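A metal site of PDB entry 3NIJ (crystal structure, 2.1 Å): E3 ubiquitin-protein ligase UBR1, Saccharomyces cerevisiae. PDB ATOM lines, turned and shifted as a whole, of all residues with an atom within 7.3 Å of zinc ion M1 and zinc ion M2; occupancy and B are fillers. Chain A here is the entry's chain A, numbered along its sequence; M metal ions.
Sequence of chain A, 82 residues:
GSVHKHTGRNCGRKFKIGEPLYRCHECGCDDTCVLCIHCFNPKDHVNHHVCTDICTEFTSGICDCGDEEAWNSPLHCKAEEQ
ND1 of His 6 is in hydrogen-bond range of O of Arg 9.
N of Cys 65 sits close to SG of Cys 63, at 3.4 Å.
O of Cys 65 lies within hydrogen-bond range of N of Cys 11.
The backbone carbonyl oxygen (O) of Cys 11 lies within hydrogen-bond range of the guanidinium group (NH2) of Arg 9 (3.1 Å).
O of Cys 39 lies within hydrogen-bond range of N of Lys 78, 3.0 Å away.
The backbone carbonyl oxygen (O) of Arg 13 is in hydrogen-bond range of the backbone NH (N) of Cys 63, 2.9 Å away.
The side-chain sulfur (SG) of Cys 11 sits close to the backbone NH (N) of Arg 13 (3.6 Å).
The backbone NH (N) of Cys 11 lies within hydrogen-bond range of a ring nitrogen (ND1) of His 6 (3.3 Å).
The nearest printed residue that does not touch zinc ion M1 is Cys 11 (4.3 Å).
Four residues have an atom within 4 Å of zinc ion M2: Cys 11, Cys 36, Cys 39 and Cys 63.
Along chain A the residues within 4 Å of zinc ion M2 span positions 11 to 63.
The nearest printed residue that does not touch zinc ion M2 is Cys 65 (4.2 Å).
Zinc ion M1 is bound by SG of Cys 77, NE2 of His 6, SG of Cys 39 and SG of Cys 65.
Zinc ion M2 is bound by SG of Cys 39, SG of Cys 63, SG of Cys 36 and SG of Cys 11.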
ATOM      1  N   HIS A   4     -10.886  13.755  30.633  1.00  0.00           N
ATOM      2  CA  HIS A   4     -11.199  12.639  29.745  1.00  0.00           C
ATOM      3  C   HIS A   4     -11.465  11.356  30.520  1.00  0.00           C
ATOM      4  O   HIS A   4     -11.761  10.313  29.931  1.00  0.00           O
ATOM      5  CB  HIS A   4     -10.067  12.442  28.744  1.00  0.00           C
ATOM      6  CG  HIS A   4      -9.524  13.727  28.186  1.00  0.00           C
ATOM      7  ND1 HIS A   4     -10.254  14.532  27.329  1.00  0.00           N
ATOM      8  CD2 HIS A   4      -8.332  14.341  28.367  1.00  0.00           C
ATOM      9  CE1 HIS A   4      -9.529  15.585  27.005  1.00  0.00           C
ATOM     10  NE2 HIS A   4      -8.358  15.494  27.621  1.00  0.00           N
ATOM     11  N   LYS A   5     -11.347  11.440  31.849  1.00  0.00           N
ATOM     12  CA  LYS A   5     -11.669  10.352  32.758  1.00  0.00           C
ATOM     13  C   LYS A   5     -13.135   9.974  32.621  1.00  0.00           C
ATOM     14  O   LYS A   5     -13.991  10.833  32.408  1.00  0.00           O
ATOM     15  CB  LYS A   5     -11.383  10.762  34.211  1.00  0.00           C
ATOM     16  CG  LYS A   5      -9.959  11.232  34.458  1.00  0.00           C
ATOM     17  CD  LYS A   5      -9.881  12.113  35.700  1.00  0.00           C
ATOM     18  CE  LYS A   5      -8.502  12.757  35.811  1.00  0.00           C
ATOM     19  NZ  LYS A   5      -8.434  13.725  36.926  1.00  0.00           N
ATOM     20  N   HIS A   6     -13.421   8.674  32.737  1.00  0.00           N
ATOM     21  CA  HIS A   6     -14.779   8.156  32.584  1.00  0.00           C
ATOM     22  C   HIS A   6     -15.013   6.923  33.454  1.00  0.00           C
ATOM     23  O   HIS A   6     -15.589   5.930  33.010  1.00  0.00           O
ATOM     24  CB  HIS A   6     -15.051   7.845  31.102  1.00  0.00           C
ATOM     25  CG  HIS A   6     -14.096   6.845  30.514  1.00  0.00           C
ATOM     26  ND1 HIS A   6     -14.363   5.492  30.516  1.00  0.00           N
ATOM     27  CD2 HIS A   6     -12.886   6.997  29.937  1.00  0.00           C
ATOM     28  CE1 HIS A   6     -13.354   4.858  29.951  1.00  0.00           C
ATOM     29  NE2 HIS A   6     -12.445   5.749  29.589  1.00  0.00           N
ATOM     30  N   ARG A   9     -17.634   3.594  33.370  1.00  0.00           N
ATOM     31  CA  ARG A   9     -18.368   3.545  32.113  1.00  0.00           C
ATOM     32  C   ARG A   9     -17.395   3.543  30.936  1.00  0.00           C
ATOM     33  O   ARG A   9     -16.191   3.754  31.113  1.00  0.00           O
ATOM     34  CB  ARG A   9     -19.385   4.686  31.993  1.00  0.00           C
ATOM     35  CG  ARG A   9     -18.827   6.098  32.233  1.00  0.00           C
ATOM     36  CD  ARG A   9     -19.682   7.167  31.539  1.00  0.00           C
ATOM     37  NE  ARG A   9     -19.377   7.245  30.093  1.00  0.00           N
ATOM     38  CZ  ARG A   9     -19.836   8.197  29.277  1.00  0.00           C
ATOM     39  NH1 ARG A   9     -20.636   9.183  29.740  1.00  0.00           N
ATOM     40  NH2 ARG A   9     -19.493   8.174  27.979  1.00  0.00           N
ATOM     41  N   ASN A  10     -17.920   3.287  29.741  1.00  0.00           N
ATOM     42  CA  ASN A  10     -17.115   3.328  28.527  1.00  0.00           C
ATOM     43  C   ASN A  10     -16.721   4.770  28.213  1.00  0.00           C
ATOM     44  O   ASN A  10     -17.392   5.717  28.639  1.00  0.00           O
ATOM     45  CB  ASN A  10     -17.896   2.731  27.362  1.00  0.00           C
ATOM     46  CG  ASN A  10     -19.094   3.584  26.965  1.00  0.00           C
ATOM     47  OD1 ASN A  10     -19.918   3.964  27.809  1.00  0.00           O
ATOM     48  ND2 ASN A  10     -19.183   3.917  25.683  1.00  0.00           N
ATOM     49  N   CYS A  11     -15.615   4.925  27.481  1.00  0.00           N
ATOM     50  CA  CYS A  11     -15.216   6.249  27.017  1.00  0.00           C
ATOM     51  C   CYS A  11     -16.229   6.773  26.002  1.00  0.00           C
ATOM     52  O   CYS A  11     -16.934   7.760  26.266  1.00  0.00           O
ATOM     53  CB  CYS A  11     -13.792   6.220  26.435  1.00  0.00           C
ATOM     54  SG  CYS A  11     -13.296   7.827  25.811  1.00  0.00           S
ATOM     55  N   GLY A  12     -16.309   6.115  24.848  1.00  0.00           N
ATOM     56  CA  GLY A  12     -17.284   6.505  23.824  1.00  0.00           C
ATOM     57  C   GLY A  12     -16.974   7.808  23.086  1.00  0.00           C
ATOM     58  O   GLY A  12     -17.802   8.287  22.304  1.00  0.00           O
ATOM     59  N   ARG A  13     -15.802   8.381  23.340  1.00  0.00           N
ATOM     60  CA  ARG A  13     -15.335   9.588  22.638  1.00  0.00           C
ATOM     61  C   ARG A  13     -15.305   9.337  21.139  1.00  0.00           C
ATOM     62  O   ARG A  13     -14.654   8.409  20.670  1.00  0.00           O
ATOM     63  CB  ARG A  13     -13.936   9.999  23.119  1.00  0.00           C
ATOM     64  CG  ARG A  13     -13.291  11.146  22.341  1.00  0.00           C
ATOM     65  CD  ARG A  13     -11.943  11.524  22.934  1.00  0.00           C
ATOM     66  NE  ARG A  13     -12.104  12.548  23.966  1.00  0.00           N
ATOM     67  CZ  ARG A  13     -12.035  13.859  23.740  1.00  0.00           C
ATOM     68  NH1 ARG A  13     -11.770  14.301  22.517  1.00  0.00           N
ATOM     69  NH2 ARG A  13     -12.200  14.724  24.739  1.00  0.00           N
ATOM     70  N   PHE A  15     -14.199   9.897  17.433  1.00  0.00           N
ATOM     71  CA  PHE A  15     -13.023  10.367  16.710  1.00  0.00           C
ATOM     72  C   PHE A  15     -13.411  11.399  15.666  1.00  0.00           C
ATOM     73  O   PHE A  15     -14.491  11.331  15.068  1.00  0.00           O
ATOM     74  CB  PHE A  15     -12.270   9.207  16.063  1.00  0.00           C
ATOM     75  CG  PHE A  15     -11.698   8.240  17.043  1.00  0.00           C
ATOM     76  CD1 PHE A  15     -10.490   8.504  17.674  1.00  0.00           C
ATOM     77  CD2 PHE A  15     -12.369   7.056  17.356  1.00  0.00           C
ATOM     78  CE1 PHE A  15      -9.963   7.610  18.606  1.00  0.00           C
ATOM     79  CE2 PHE A  15     -11.842   6.153  18.276  1.00  0.00           C
ATOM     80  CZ  PHE A  15     -10.640   6.424  18.911  1.00  0.00           C
ATOM     81  N   VAL A  34     -10.903  -0.045  19.338  1.00  0.00           N
ATOM     82  CA  VAL A  34      -9.994   1.105  19.275  1.00  0.00           C
ATOM     83  C   VAL A  34      -9.949   1.932  20.565  1.00  0.00           C
ATOM     84  O   VAL A  34     -10.909   1.951  21.348  1.00  0.00           O
ATOM     85  CB  VAL A  34     -10.330   2.062  18.080  1.00  0.00           C
ATOM     86  CG1 VAL A  34     -10.235   1.340  16.742  1.00  0.00           C
ATOM     87  CG2 VAL A  34     -11.732   2.660  18.238  1.00  0.00           C
ATOM     88  N   LEU A  35      -8.838   2.645  20.750  1.00  0.00           N
ATOM     89  CA  LEU A  35      -8.606   3.545  21.887  1.00  0.00           C
ATOM     90  C   LEU A  35      -8.220   4.934  21.387  1.00  0.00           C
ATOM     91  O   LEU A  35      -7.499   5.066  20.404  1.00  0.00           O
ATOM     92  CB  LEU A  35      -7.482   3.015  22.772  1.00  0.00           C
ATOM     93  CG  LEU A  35      -7.717   1.697  23.529  1.00  0.00           C
ATOM     94  CD1 LEU A  35      -6.404   1.069  23.963  1.00  0.00           C
ATOM     95  CD2 LEU A  35      -8.626   1.921  24.721  1.00  0.00           C
ATOM     96  N   CYS A  36      -8.701   5.971  22.071  1.00  0.00           N
ATOM     97  CA  CYS A  36      -8.281   7.337  21.755  1.00  0.00           C
ATOM     98  C   CYS A  36      -6.947   7.668  22.418  1.00  0.00           C
ATOM     99  O   CYS A  36      -6.448   6.889  23.244  1.00  0.00           O
ATOM    100  CB  CYS A  36      -9.356   8.357  22.128  1.00  0.00           C
ATOM    101  SG  CYS A  36      -9.579   8.626  23.898  1.00  0.00           S
ATOM    102  N   ILE A  37      -6.385   8.831  22.072  1.00  0.00           N
ATOM    103  CA  ILE A  37      -5.091   9.276  22.585  1.00  0.00           C
ATOM    104  C   ILE A  37      -5.141   9.562  24.093  1.00  0.00           C
ATOM    105  O   ILE A  37      -4.146   9.417  24.790  1.00  0.00           O
ATOM    106  CB  ILE A  37      -4.525  10.491  21.761  1.00  0.00           C
ATOM    107  CG1 ILE A  37      -3.034  10.713  22.074  1.00  0.00           C
ATOM    108  CG2 ILE A  37      -5.368  11.764  21.985  1.00  0.00           C
ATOM    109  CD1 ILE A  37      -2.296  11.630  21.096  1.00  0.00           C
ATOM    110  N   HIS A  38      -6.314   9.959  24.587  1.00  0.00           N
ATOM    111  CA  HIS A  38      -6.482  10.243  26.009  1.00  0.00           C
ATOM    112  C   HIS A  38      -6.622   8.975  26.858  1.00  0.00           C
ATOM    113  O   HIS A  38      -6.480   9.032  28.088  1.00  0.00           O
ATOM    114  CB  HIS A  38      -7.685  11.161  26.224  1.00  0.00           C
ATOM    115  CG  HIS A  38      -7.620  12.434  25.429  1.00  0.00           C
ATOM    116  ND1 HIS A  38      -8.544  12.754  24.461  1.00  0.00           N
ATOM    117  CD2 HIS A  38      -6.712  13.439  25.451  1.00  0.00           C
ATOM    118  CE1 HIS A  38      -8.225  13.917  23.923  1.00  0.00           C
ATOM    119  NE2 HIS A  38      -7.115  14.354  24.497  1.00  0.00           N
ATOM    120  N   CYS A  39      -6.895   7.845  26.202  1.00  0.00           N
ATOM    121  CA  CYS A  39      -7.194   6.593  26.888  1.00  0.00           C
ATOM    122  C   CYS A  39      -6.052   5.571  26.745  1.00  0.00           C
ATOM    123  O   CYS A  39      -5.735   4.830  27.686  1.00  0.00           O
ATOM    124  CB  CYS A  39      -8.509   5.998  26.355  1.00  0.00           C
ATOM    125  SG  CYS A  39     -10.085   6.899  26.738  1.00  0.00           S
ATOM    126  N   PHE A  40      -5.433   5.532  25.559  1.00  0.00           N
ATOM    127  CA  PHE A  40      -4.333   4.612  25.286  1.00  0.00           C
ATOM    128  C   PHE A  40      -3.152   4.797  26.244  1.00  0.00           C
ATOM    129  O   PHE A  40      -2.570   5.886  26.348  1.00  0.00           O
ATOM    130  CB  PHE A  40      -3.863   4.726  23.830  1.00  0.00           C
ATOM    131  CG  PHE A  40      -2.701   3.821  23.468  1.00  0.00           C
ATOM    132  CD1 PHE A  40      -2.914   2.497  23.120  1.00  0.00           C
ATOM    133  CD2 PHE A  40      -1.394   4.309  23.482  1.00  0.00           C
ATOM    134  CE1 PHE A  40      -1.839   1.663  22.776  1.00  0.00           C
ATOM    135  CE2 PHE A  40      -0.312   3.486  23.156  1.00  0.00           C
ATOM    136  CZ  PHE A  40      -0.548   2.158  22.804  1.00  0.00           C
ATOM    137  N   ILE A  62     -15.966   5.402  17.626  1.00  0.00           N
ATOM    138  CA  ILE A  62     -15.816   5.806  19.026  1.00  0.00           C
ATOM    139  C   ILE A  62     -14.780   4.976  19.789  1.00  0.00           C
ATOM    140  O   ILE A  62     -14.535   3.819  19.456  1.00  0.00           O
ATOM    141  CB  ILE A  62     -17.170   5.768  19.800  1.00  0.00           C
ATOM    142  CG1 ILE A  62     -17.764   4.355  19.802  1.00  0.00           C
ATOM    143  CG2 ILE A  62     -18.161   6.786  19.219  1.00  0.00           C
ATOM    144  CD1 ILE A  62     -18.747   4.073  20.932  1.00  0.00           C
ATOM    145  N   CYS A  63     -14.201   5.581  20.817  1.00  0.00           N
ATOM    146  CA  CYS A  63     -13.220   4.917  21.665  1.00  0.00           C
ATOM    147  C   CYS A  63     -13.898   3.816  22.489  1.00  0.00           C
ATOM    148  O   CYS A  63     -14.998   4.018  23.014  1.00  0.00           O
ATOM    149  CB  CYS A  63     -12.531   5.917  22.587  1.00  0.00           C
ATOM    150  SG  CYS A  63     -11.467   5.145  23.808  1.00  0.00           S
ATOM    151  N   ASP A  64     -13.234   2.668  22.602  1.00  0.00           N
ATOM    152  CA  ASP A  64     -13.771   1.492  23.290  1.00  0.00           C
ATOM    153  C   ASP A  64     -13.243   1.278  24.703  1.00  0.00           C
ATOM    154  O   ASP A  64     -13.605   0.296  25.368  1.00  0.00           O
ATOM    155  CB  ASP A  64     -13.560   0.225  22.451  1.00  0.00           C
ATOM    156  CG  ASP A  64     -14.249   0.300  21.115  1.00  0.00           C
ATOM    157  OD1 ASP A  64     -15.453   0.593  21.097  1.00  0.00           O
ATOM    158  OD2 ASP A  64     -13.594   0.074  20.076  1.00  0.00           O
ATOM    159  N   CYS A  65     -12.403   2.203  25.174  1.00  0.00           N
ATOM    160  CA  CYS A  65     -11.884   2.118  26.544  1.00  0.00           C
ATOM    161  C   CYS A  65     -13.025   1.990  27.551  1.00  0.00           C
ATOM    162  O   CYS A  65     -13.962   2.793  27.554  1.00  0.00           O
ATOM    163  CB  CYS A  65     -11.050   3.347  26.889  1.00  0.00           C
ATOM    164  SG  CYS A  65     -10.095   3.158  28.402  1.00  0.00           S
ATOM    165  N   GLY A  66     -12.960   0.965  28.390  1.00  0.00           N
ATOM    166  CA  GLY A  66     -13.987   0.722  29.397  1.00  0.00           C
ATOM    167  C   GLY A  66     -15.168  -0.125  28.940  1.00  0.00           C
ATOM    168  O   GLY A  66     -16.048  -0.441  29.733  1.00  0.00           O
ATOM    169  N   HIS A  76      -5.912  -0.023  31.557  1.00  0.00           N
ATOM    170  CA  HIS A  76      -5.759   0.987  32.595  1.00  0.00           C
ATOM    171  C   HIS A  76      -5.694   2.363  31.936  1.00  0.00           C
ATOM    172  O   HIS A  76      -4.618   2.812  31.522  1.00  0.00           O
ATOM    173  CB  HIS A  76      -4.497   0.721  33.429  1.00  0.00           C
ATOM    174  CG  HIS A  76      -4.449  -0.649  34.024  1.00  0.00           C
ATOM    175  ND1 HIS A  76      -4.927  -0.927  35.284  1.00  0.00           N
ATOM    176  CD2 HIS A  76      -3.978  -1.823  33.530  1.00  0.00           C
ATOM    177  CE1 HIS A  76      -4.748  -2.210  35.551  1.00  0.00           C
ATOM    178  NE2 HIS A  76      -4.179  -2.776  34.496  1.00  0.00           N
ATOM    179  N   CYS A  77      -6.867   3.000  31.831  1.00  0.00           N
ATOM    180  CA  CYS A  77      -7.057   4.296  31.166  1.00  0.00           C
ATOM    181  C   CYS A  77      -5.951   5.295  31.509  1.00  0.00           C
ATOM    182  O   CYS A  77      -5.686   5.556  32.691  1.00  0.00           O
ATOM    183  CB  CYS A  77      -8.436   4.879  31.559  1.00  0.00           C
ATOM    184  SG  CYS A  77      -9.201   6.012  30.345  1.00  0.00           S
ATOM    185  N   LYS A  78      -5.314   5.849  30.479  1.00  0.00           N
ATOM    186  CA  LYS A  78      -4.261   6.857  30.659  1.00  0.00           C
ATOM    187  C   LYS A  78      -4.774   8.122  31.347  1.00  0.00           C
ATOM    188  O   LYS A  78      -4.060   8.742  32.135  1.00  0.00           O
ATOM    189  CB  LYS A  78      -3.597   7.220  29.328  1.00  0.00           C
ATOM    190  CG  LYS A  78      -2.177   7.752  29.475  1.00  0.00           C
ATOM    191  CD  LYS A  78      -1.881   8.892  28.506  1.00  0.00           C
ATOM    192  CE  LYS A  78      -0.454   9.400  28.681  1.00  0.00           C
ATOM    193  NZ  LYS A  78      -0.291  10.812  28.201  1.00  0.00           N
ATOM    194  N   ALA A  79      -6.011   8.507  31.040  1.00  0.00           N
ATOM    195  CA  ALA A  79      -6.656   9.673  31.669  1.00  0.00           C
ATOM    196  C   ALA A  79      -6.831   9.472  33.185  1.00  0.00           C
ATOM    197  O   ALA A  79      -6.838  10.449  33.935  1.00  0.00           O
ATOM    198  CB  ALA A  79      -7.990   9.966  31.019  1.00  0.00           C
ATOM    199  N   GLU A  80      -6.939   8.216  33.598  1.00  0.00           N
ATOM    200  CA  GLU A  80      -7.206   7.853  34.995  1.00  0.00           C
ATOM    201  C   GLU A  80      -5.980   8.001  35.908  1.00  0.00           C
ATOM    202  O   GLU A  80      -6.119   8.054  37.135  1.00  0.00           O
ATOM    203  CB  GLU A  80      -7.753   6.430  35.068  1.00  0.00           C
ATOM    204  CG  GLU A  80      -8.775   6.188  36.166  1.00  0.00           C
ATOM    205  CD  GLU A  80      -9.922   7.187  36.125  1.00  0.00           C
ATOM    206  OE1 GLU A  80     -10.655   7.214  35.109  1.00  0.00           O
ATOM    207  OE2 GLU A  80     -10.093   7.927  37.110  1.00  0.00           O
HETATM  208 ZN    ZN M   1     -10.240   5.655  28.750  1.00  0.00          ZN
HETATM  209 ZN    ZN M   2     -11.122   7.103  24.948  1.00  0.00          ZN
